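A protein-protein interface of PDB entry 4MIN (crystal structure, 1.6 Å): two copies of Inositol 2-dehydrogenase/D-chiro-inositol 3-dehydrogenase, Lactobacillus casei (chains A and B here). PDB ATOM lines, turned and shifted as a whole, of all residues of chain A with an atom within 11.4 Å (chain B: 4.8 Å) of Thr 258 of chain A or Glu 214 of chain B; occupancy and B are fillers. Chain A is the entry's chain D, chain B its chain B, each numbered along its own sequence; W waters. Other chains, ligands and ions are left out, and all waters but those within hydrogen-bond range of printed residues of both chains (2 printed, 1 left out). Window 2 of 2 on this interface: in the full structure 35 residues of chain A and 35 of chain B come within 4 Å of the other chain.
Asp 153 of chain A touches none of the printed residues of chain B. Ile 255 of chain A touches none of the printed residues of chain B. Of the printed residues of chain B, Glu 257 of chain A touches Ser 212 (3.5 Å), Ala 213 (3.1 Å), Glu 214 (3.8 Å), Thr 243 (3.4 Å), Ala 244 (3.6 Å) and Gln 245 (3.8 Å). Of the printed residues of chain B, Gly 259 of chain A touches Ala 244 (3.8 Å). Of the printed residues of chain B, Glu 260 of chain A touches Tyr 246 (3.7 Å). Of chain A, only Glu 257 comes within 4 Å of Ser 212 of chain B. Of chain A, only Glu 257 comes within 4 Å of Ala 213 of chain B. Of chain A, only Glu 257 (3.8 Å) and Thr 258 (3.3 Å) come within 4 Å of Glu 214 of chain B. Val 215 of chain B touches none of the printed residues of chain A. Of chain A, only Glu 257 comes within 4 Å of Thr 243 of chain B. Of chain A, only Glu 257, Thr 258 and Gly 259 come within 4 Å of Ala 244 of chain B. Gln 245 of chain B touches just these residues of chain A: Glu 257 and Thr 258. Printed residues of chain A within 4 Å of Tyr 246 of chain B: Glu 260 (3.7 Å). The nearest printed residue of chain B that does not touch Glu 257 of chain A is Tyr 246 of chain B (6.2 Å).
No position is printed for both chains.
Water W2 lies within hydrogen-bond range of the side-chain hydroxyl of Ser 212 of chain B, the backbone carbonyl oxygen of Thr 243 of chain B and the backbone carbonyl oxygen of Glu 257 of chain A. Water W1 lies within hydrogen-bond range of OE1 of Glu 257 of chain A and OE2 of Glu 214 of chain B.
The backbone NH of Ala 213 of chain B lies within hydrogen-bond range of the side-chain carboxylate of Glu 257 of chain A. O of Glu 257 of chain A sits close to O of Thr 243 of chain B (3.4 Å).
Printed residues of chain B that touch a printed residue of chain A: Ser 212, Ala 213, Glu 214, Thr 243, Ala 244, Gln 245 and Tyr 246. Hydrophobic or aromatic side chains of chain B that line the printed part of chain A: Ala 213 and Tyr 246. Printed residues of chain A that touch a printed residue of chain B: Glu 257, Thr 258, Gly 259 and Glu 260. Among the printed residues, no Asp or Glu carboxylate lies within 4 Å of a Lys or Arg side-chain nitrogen of the other chain.
The side-chain hydroxyl (OG) of Ser 212 of chain B sits close to the backbone NH (N) of Glu 214 of chain B. The backbone carbonyl oxygen of Thr 243 of chain B sits at hydrogen-bond distance from the side-chain amide nitrogen of Gln 245 of chain B (3.0 Å). N of Ala 159 of chain A is in hydrogen-bond range of OE1 of Glu 257 of chain A, at 2.9 Å. The backbone carbonyl oxygen (O) of Ile 156 of chain A is in hydrogen-bond range of the side-chain hydroxyl (OG1) of Thr 258 of chain A (3.3 Å). The backbone carbonyl oxygen of Ile 157 of chain A sits at hydrogen-bond distance from the backbone NH of Thr 258 of chain A (3.0 Å). The backbone NH (N) of Glu 257 of chain A sits at hydrogen-bond distance from the backbone carbonyl oxygen (O) of Ile 157 of chain A.
Among the printed residues, pairs that only touch across the chains: Glu 257 of chain A with Ser 212 of chain B, Glu 257 of chain A with Glu 214 of chain B, Glu 257 of chain A with Ala 244 of chain B, Glu 257 of chain A with Gln 245 of chain B, Thr 258 of chain A with Glu 214 of chain B, Thr 258 of chain A with Ala 244 of chain B, Thr 258 of chain A with Gln 245 of chain B, Gly 259 of chain A with Ala 244 of chain B and Glu 260 of chain A with Tyr 246 of chain B.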
ATOM      1  N   LYS A 151       6.712  24.755 -25.192  1.00  0.00           N
ATOM      2  CA  LYS A 151       5.982  24.563 -23.945  1.00  0.00           C
ATOM      3  C   LYS A 151       6.548  23.430 -23.135  1.00  0.00           C
ATOM      4  O   LYS A 151       6.643  23.511 -21.933  1.00  0.00           O
ATOM      5  CB  LYS A 151       4.505  24.330 -24.215  1.00  0.00           C
ATOM      6  CG  LYS A 151       3.577  24.486 -23.028  1.00  0.00           C
ATOM      7  CD  LYS A 151       3.419  25.895 -22.605  1.00  0.00           C
ATOM      8  CE  LYS A 151       2.354  26.037 -21.527  1.00  0.00           C
ATOM      9  NZ  LYS A 151       2.410  27.416 -20.967  1.00  0.00           N
ATOM     10  N   LEU A 152       6.942  22.374 -23.809  1.00  0.00           N
ATOM     11  CA  LEU A 152       7.536  21.237 -23.150  1.00  0.00           C
ATOM     12  C   LEU A 152       8.769  21.672 -22.410  1.00  0.00           C
ATOM     13  O   LEU A 152       9.005  21.271 -21.312  1.00  0.00           O
ATOM     14  CB  LEU A 152       7.920  20.202 -24.184  1.00  0.00           C
ATOM     15  CG  LEU A 152       8.694  18.977 -23.716  1.00  0.00           C
ATOM     16  CD1 LEU A 152       7.878  18.173 -22.766  1.00  0.00           C
ATOM     17  CD2 LEU A 152       9.127  18.124 -24.875  1.00  0.00           C
ATOM     18  N   ASP A 153       9.542  22.490 -23.081  1.00  0.00           N
ATOM     19  CA  ASP A 153      10.825  22.911 -22.573  1.00  0.00           C
ATOM     20  C   ASP A 153      10.723  23.878 -21.410  1.00  0.00           C
ATOM     21  O   ASP A 153      11.690  24.136 -20.775  1.00  0.00           O
ATOM     22  CB  ASP A 153      11.707  23.457 -23.705  1.00  0.00           C
ATOM     23  CG  ASP A 153      12.133  22.375 -24.655  1.00  0.00           C
ATOM     24  OD1 ASP A 153      12.046  21.217 -24.275  1.00  0.00           O
ATOM     25  OD2 ASP A 153      12.572  22.678 -25.760  1.00  0.00           O
ATOM     26  N   THR A 154       9.542  24.375 -21.112  1.00  0.00           N
ATOM     27  CA  THR A 154       9.397  25.195 -19.932  1.00  0.00           C
ATOM     28  C   THR A 154       9.338  24.402 -18.646  1.00  0.00           C
ATOM     29  O   THR A 154       9.410  24.971 -17.589  1.00  0.00           O
ATOM     30  CB  THR A 154       8.135  26.048 -19.922  1.00  0.00           C
ATOM     31  OG1 THR A 154       6.988  25.208 -19.903  1.00  0.00           O
ATOM     32  CG2 THR A 154       8.073  26.921 -21.115  1.00  0.00           C
ATOM     33  N   GLY A 155       9.143  23.110 -18.764  1.00  0.00           N
ATOM     34  CA  GLY A 155       9.030  22.274 -17.611  1.00  0.00           C
ATOM     35  C   GLY A 155       7.646  22.091 -17.036  1.00  0.00           C
ATOM     36  O   GLY A 155       7.484  21.427 -16.065  1.00  0.00           O
ATOM     37  N   ILE A 156       6.668  22.659 -17.682  1.00  0.00           N
ATOM     38  CA  ILE A 156       5.331  22.694 -17.151  1.00  0.00           C
ATOM     39  C   ILE A 156       4.719  21.296 -16.952  1.00  0.00           C
ATOM     40  O   ILE A 156       3.936  21.120 -16.068  1.00  0.00           O
ATOM     41  CB  ILE A 156       4.430  23.660 -17.965  1.00  0.00           C
ATOM     42  CG1 ILE A 156       3.082  23.854 -17.327  1.00  0.00           C
ATOM     43  CG2 ILE A 156       4.125  23.150 -19.286  1.00  0.00           C
ATOM     44  CD1 ILE A 156       3.090  24.571 -16.227  1.00  0.00           C
ATOM     45  N   ILE A 157       5.114  20.320 -17.751  1.00  0.00           N
ATOM     46  CA  ILE A 157       4.602  18.972 -17.584  1.00  0.00           C
ATOM     47  C   ILE A 157       5.616  17.962 -17.061  1.00  0.00           C
ATOM     48  O   ILE A 157       5.384  16.805 -17.074  1.00  0.00           O
ATOM     49  CB  ILE A 157       3.964  18.405 -18.880  1.00  0.00           C
ATOM     50  CG1 ILE A 157       4.991  18.222 -19.987  1.00  0.00           C
ATOM     51  CG2 ILE A 157       2.866  19.274 -19.318  1.00  0.00           C
ATOM     52  CD1 ILE A 157       4.424  17.454 -21.166  1.00  0.00           C
ATOM     53  N   GLY A 158       6.747  18.466 -16.610  1.00  0.00           N
ATOM     54  CA  GLY A 158       7.801  17.606 -16.152  1.00  0.00           C
ATOM     55  C   GLY A 158       8.518  16.955 -17.289  1.00  0.00           C
ATOM     56  O   GLY A 158       8.463  17.432 -18.387  1.00  0.00           O
ATOM     57  N   ALA A 159       9.177  15.850 -16.989  1.00  0.00           N
ATOM     58  CA  ALA A 159       9.953  15.107 -17.960  1.00  0.00           C
ATOM     59  C   ALA A 159       9.053  14.329 -18.918  1.00  0.00           C
ATOM     60  O   ALA A 159       8.047  13.825 -18.534  1.00  0.00           O
ATOM     61  CB  ALA A 159      10.872  14.151 -17.282  1.00  0.00           C
ATOM     62  N   PRO A 160       9.461  14.251 -20.175  1.00  0.00           N
ATOM     63  CA  PRO A 160       8.697  13.446 -21.103  1.00  0.00           C
ATOM     64  C   PRO A 160       8.943  11.951 -20.930  1.00  0.00           C
ATOM     65  O   PRO A 160      10.039  11.501 -21.019  1.00  0.00           O
ATOM     66  CB  PRO A 160       9.197  13.934 -22.458  1.00  0.00           C
ATOM     67  CG  PRO A 160      10.566  14.422 -22.179  1.00  0.00           C
ATOM     68  CD  PRO A 160      10.543  14.978 -20.830  1.00  0.00           C
ATOM     69  N   LEU A 161       7.881  11.218 -20.690  1.00  0.00           N
ATOM     70  CA  LEU A 161       7.985   9.814 -20.451  1.00  0.00           C
ATOM     71  C   LEU A 161       7.645   9.001 -21.679  1.00  0.00           C
ATOM     72  O   LEU A 161       8.292   8.038 -21.979  1.00  0.00           O
ATOM     73  CB  LEU A 161       7.044   9.414 -19.321  1.00  0.00           C
ATOM     74  CG  LEU A 161       7.149  10.301 -18.090  1.00  0.00           C
ATOM     75  CD1 LEU A 161       6.035  10.124 -17.118  1.00  0.00           C
ATOM     76  CD2 LEU A 161       8.429  10.060 -17.401  1.00  0.00           C
ATOM     77  N   VAL A 162       6.575   9.409 -22.340  1.00  0.00           N
ATOM     78  CA  VAL A 162       6.049   8.685 -23.491  1.00  0.00           C
ATOM     79  C   VAL A 162       5.597   9.697 -24.546  1.00  0.00           C
ATOM     80  O   VAL A 162       5.087  10.707 -24.210  1.00  0.00           O
ATOM     81  CB  VAL A 162       4.841   7.791 -23.113  1.00  0.00           C
ATOM     82  CG1 VAL A 162       4.226   7.177 -24.338  1.00  0.00           C
ATOM     83  CG2 VAL A 162       5.253   6.685 -22.185  1.00  0.00           C
ATOM     84  N   VAL A 254       2.561  14.424 -26.094  1.00  0.00           N
ATOM     85  CA  VAL A 254       3.622  14.186 -25.163  1.00  0.00           C
ATOM     86  C   VAL A 254       3.098  13.987 -23.733  1.00  0.00           C
ATOM     87  O   VAL A 254       2.480  14.832 -23.193  1.00  0.00           O
ATOM     88  CB  VAL A 254       4.644  15.316 -25.144  1.00  0.00           C
ATOM     89  CG1 VAL A 254       5.710  15.009 -24.119  1.00  0.00           C
ATOM     90  CG2 VAL A 254       5.245  15.455 -26.487  1.00  0.00           C
ATOM     91  N   ILE A 255       3.401  12.824 -23.188  1.00  0.00           N
ATOM     92  CA  ILE A 255       3.005  12.467 -21.845  1.00  0.00           C
ATOM     93  C   ILE A 255       4.154  12.766 -20.873  1.00  0.00           C
ATOM     94  O   ILE A 255       5.182  12.174 -20.949  1.00  0.00           O
ATOM     95  CB  ILE A 255       2.551  10.988 -21.772  1.00  0.00           C
ATOM     96  CG1 ILE A 255       1.246  10.816 -22.554  1.00  0.00           C
ATOM     97  CG2 ILE A 255       2.292  10.556 -20.345  1.00  0.00           C
ATOM     98  CD1 ILE A 255       1.399  10.077 -23.718  1.00  0.00           C
ATOM     99  N   GLY A 256       3.922  13.703 -19.976  1.00  0.00           N
ATOM    100  CA  GLY A 256       4.901  14.089 -18.995  1.00  0.00           C
ATOM    101  C   GLY A 256       4.508  13.624 -17.607  1.00  0.00           C
ATOM    102  O   GLY A 256       3.457  13.134 -17.404  1.00  0.00           O
ATOM    103  N   GLU A 257       5.419  13.840 -16.678  1.00  0.00           N
ATOM    104  CA  GLU A 257       5.249  13.456 -15.310  1.00  0.00           C
ATOM    105  C   GLU A 257       4.045  14.110 -14.668  1.00  0.00           C
ATOM    106  O   GLU A 257       3.406  13.527 -13.875  1.00  0.00           O
ATOM    107  CB  GLU A 257       6.524  13.783 -14.531  1.00  0.00           C
ATOM    108  CG  GLU A 257       7.698  12.952 -14.945  1.00  0.00           C
ATOM    109  CD  GLU A 257       9.031  13.444 -14.380  1.00  0.00           C
ATOM    110  OE1 GLU A 257       9.250  14.643 -14.299  1.00  0.00           O
ATOM    111  OE2 GLU A 257       9.858  12.583 -14.049  1.00  0.00           O
ATOM    112  N   THR A 258       3.785  15.349 -15.020  1.00  0.00           N
ATOM    113  CA  THR A 258       2.776  16.117 -14.326  1.00  0.00           C
ATOM    114  C   THR A 258       1.677  16.681 -15.198  1.00  0.00           C
ATOM    115  O   THR A 258       0.824  17.388 -14.748  1.00  0.00           O
ATOM    116  CB  THR A 258       3.406  17.279 -13.548  1.00  0.00           C
ATOM    117  OG1 THR A 258       3.880  18.258 -14.448  1.00  0.00           O
ATOM    118  CG2 THR A 258       4.520  16.762 -12.663  1.00  0.00           C
ATOM    119  N   GLY A 259       1.718  16.298 -16.458  1.00  0.00           N
ATOM    120  CA  GLY A 259       0.744  16.736 -17.416  1.00  0.00           C
ATOM    121  C   GLY A 259       0.998  16.202 -18.795  1.00  0.00           C
ATOM    122  O   GLY A 259       1.883  15.426 -18.977  1.00  0.00           O
ATOM    123  N   GLU A 260       0.176  16.633 -19.737  1.00  0.00           N
ATOM    124  CA  GLU A 260       0.308  16.244 -21.128  1.00  0.00           C
ATOM    125  C   GLU A 260       0.228  17.451 -22.043  1.00  0.00           C
ATOM    126  O   GLU A 260      -0.376  18.408 -21.727  1.00  0.00           O
ATOM    127  CB  GLU A 260      -0.772  15.234 -21.535  1.00  0.00           C
ATOM    128  CG  GLU A 260      -0.751  13.935 -20.798  1.00  0.00           C
ATOM    129  CD  GLU A 260      -1.808  12.941 -21.278  1.00  0.00           C
ATOM    130  OE1 GLU A 260      -2.547  13.300 -22.183  1.00  0.00           O
ATOM    131  OE2 GLU A 260      -1.878  11.838 -20.740  1.00  0.00           O
ATOM    132  N   LEU A 261       0.886  17.339 -23.187  1.00  0.00           N
ATOM    133  CA  LEU A 261       0.801  18.311 -24.239  1.00  0.00           C
ATOM    134  C   LEU A 261       0.393  17.670 -25.576  1.00  0.00           C
ATOM    135  O   LEU A 261       0.851  16.631 -25.926  1.00  0.00           O
ATOM    136  CB  LEU A 261       2.130  19.041 -24.397  1.00  0.00           C
ATOM    137  CG  LEU A 261       2.501  20.105 -23.367  1.00  0.00           C
ATOM    138  CD1 LEU A 261       3.946  20.468 -23.428  1.00  0.00           C
ATOM    139  CD2 LEU A 261       1.703  21.352 -23.530  1.00  0.00           C
ATOM    140  N   SER B 212       8.674   7.625 -13.731  1.00  0.00           N
ATOM    141  CA  SER B 212       8.297   8.945 -13.310  1.00  0.00           C
ATOM    142  C   SER B 212       8.839   9.330 -11.933  1.00  0.00           C
ATOM    143  O   SER B 212       8.792   8.549 -11.014  1.00  0.00           O
ATOM    144  CB  SER B 212       6.788   9.090 -13.248  1.00  0.00           C
ATOM    145  OG  SER B 212       6.463  10.396 -12.882  1.00  0.00           O
ATOM    146  N   ALA B 213       9.277  10.569 -11.826  1.00  0.00           N
ATOM    147  CA  ALA B 213       9.704  11.109 -10.553  1.00  0.00           C
ATOM    148  C   ALA B 213       8.557  11.260  -9.541  1.00  0.00           C
ATOM    149  O   ALA B 213       8.802  11.447  -8.369  1.00  0.00           O
ATOM    150  CB  ALA B 213      10.388  12.379 -10.737  1.00  0.00           C
ATOM    151  N   GLU B 214       7.325  11.164 -10.007  1.00  0.00           N
ATOM    152  CA  GLU B 214       6.188  11.311  -9.123  1.00  0.00           C
ATOM    153  C   GLU B 214       5.829  10.057  -8.358  1.00  0.00           C
ATOM    154  O   GLU B 214       4.994  10.077  -7.508  1.00  0.00           O
ATOM    155  CB  GLU B 214       4.983  11.802  -9.865  1.00  0.00           C
ATOM    156  CG  GLU B 214       5.191  13.093 -10.572  1.00  0.00           C
ATOM    157  CD  GLU B 214       5.276  14.287  -9.660  1.00  0.00           C
ATOM    158  OE1 GLU B 214       4.765  14.220  -8.560  1.00  0.00           O
ATOM    159  OE2 GLU B 214       5.851  15.276 -10.067  1.00  0.00           O
ATOM    160  N   VAL B 215       6.474   8.962  -8.670  1.00  0.00           N
ATOM    161  CA  VAL B 215       6.209   7.743  -7.960  1.00  0.00           C
ATOM    162  C   VAL B 215       6.764   7.763  -6.549  1.00  0.00           C
ATOM    163  O   VAL B 215       7.921   7.995  -6.358  1.00  0.00           O
ATOM    164  CB  VAL B 215       6.793   6.585  -8.670  1.00  0.00           C
ATOM    165  CG1 VAL B 215       6.675   5.357  -7.853  1.00  0.00           C
ATOM    166  CG2 VAL B 215       6.110   6.431 -10.042  1.00  0.00           C
ATOM    167  N   ARG B 216       5.889   7.514  -5.595  1.00  0.00           N
ATOM    168  CA  ARG B 216       6.258   7.421  -4.189  1.00  0.00           C
ATOM    169  C   ARG B 216       6.052   6.015  -3.599  1.00  0.00           C
ATOM    170  O   ARG B 216       6.222   5.827  -2.420  1.00  0.00           O
ATOM    171  CB  ARG B 216       5.466   8.431  -3.383  1.00  0.00           C
ATOM    172  CG  ARG B 216       5.795   9.864  -3.674  1.00  0.00           C
ATOM    173  CD  ARG B 216       7.235  10.165  -3.409  1.00  0.00           C
ATOM    174  NE  ARG B 216       7.472  11.513  -2.908  1.00  0.00           N
ATOM    175  CZ  ARG B 216       7.910  11.810  -1.673  1.00  0.00           C
ATOM    176  NH1 ARG B 216       8.160  10.857  -0.775  1.00  0.00           N
ATOM    177  NH2 ARG B 216       8.109  13.061  -1.317  1.00  0.00           N
ATOM    178  N   THR B 243       0.299   8.170 -11.774  1.00  0.00           N
ATOM    179  CA  THR B 243       0.772   9.335 -11.050  1.00  0.00           C
ATOM    180  C   THR B 243       0.854  10.574 -11.940  1.00  0.00           C
ATOM    181  O   THR B 243       1.712  11.371 -11.817  1.00  0.00           O
ATOM    182  CB  THR B 243       2.113   9.070 -10.415  1.00  0.00           C
ATOM    183  OG1 THR B 243       3.100   8.904 -11.427  1.00  0.00           O
ATOM    184  CG2 THR B 243       2.017   7.841  -9.609  1.00  0.00           C
ATOM    185  N   ALA B 244      -0.133  10.688 -12.811  1.00  0.00           N
ATOM    186  CA  ALA B 244      -0.142  11.689 -13.863  1.00  0.00           C
ATOM    187  C   ALA B 244      -0.379  13.120 -13.423  1.00  0.00           C
ATOM    188  O   ALA B 244      -0.175  14.025 -14.150  1.00  0.00           O
ATOM    189  CB  ALA B 244      -1.176  11.312 -14.863  1.00  0.00           C
ATOM    190  N   GLN B 245      -0.884  13.245 -12.209  1.00  0.00           N
ATOM    191  CA  GLN B 245      -1.132  14.521 -11.554  1.00  0.00           C
ATOM    192  C   GLN B 245      -2.312  15.328 -12.034  1.00  0.00           C
ATOM    193  O   GLN B 245      -3.048  15.830 -11.271  1.00  0.00           O
ATOM    194  CB  GLN B 245       0.109  15.416 -11.528  1.00  0.00           C
ATOM    195  CG  GLN B 245       1.331  14.783 -10.939  1.00  0.00           C
ATOM    196  CD  GLN B 245       1.109  14.268  -9.528  1.00  0.00           C
ATOM    197  OE1 GLN B 245       0.720  14.987  -8.651  1.00  0.00           O
ATOM    198  NE2 GLN B 245       1.340  13.014  -9.351  1.00  0.00           N
ATOM    199  N   TYR B 246      -2.474  15.428 -13.328  1.00  0.00           N
ATOM    200  CA  TYR B 246      -3.394  16.424 -13.828  1.00  0.00           C
ATOM    201  C   TYR B 246      -4.875  16.068 -13.689  1.00  0.00           C
ATOM    202  O   TYR B 246      -5.699  16.927 -13.675  1.00  0.00           O
ATOM    203  CB  TYR B 246      -3.114  16.742 -15.291  1.00  0.00           C
ATOM    204  CG  TYR B 246      -3.634  15.754 -16.314  1.00  0.00           C
ATOM    205  CD1 TYR B 246      -4.918  15.811 -16.776  1.00  0.00           C
ATOM    206  CD2 TYR B 246      -2.809  14.816 -16.847  1.00  0.00           C
ATOM    207  CE1 TYR B 246      -5.360  14.936 -17.683  1.00  0.00           C
ATOM    208  CE2 TYR B 246      -3.242  13.957 -17.757  1.00  0.00           C
ATOM    209  CZ  TYR B 246      -4.512  14.001 -18.186  1.00  0.00           C
ATOM    210  OH  TYR B 246      -4.942  13.103 -19.112  1.00  0.00           O
HETATM  211  O   HOH W   1       8.085  16.268 -12.228  1.00  0.00           O
HETATM  212  O   HOH W   2       3.928  10.762 -13.392  1.00  0.00           O
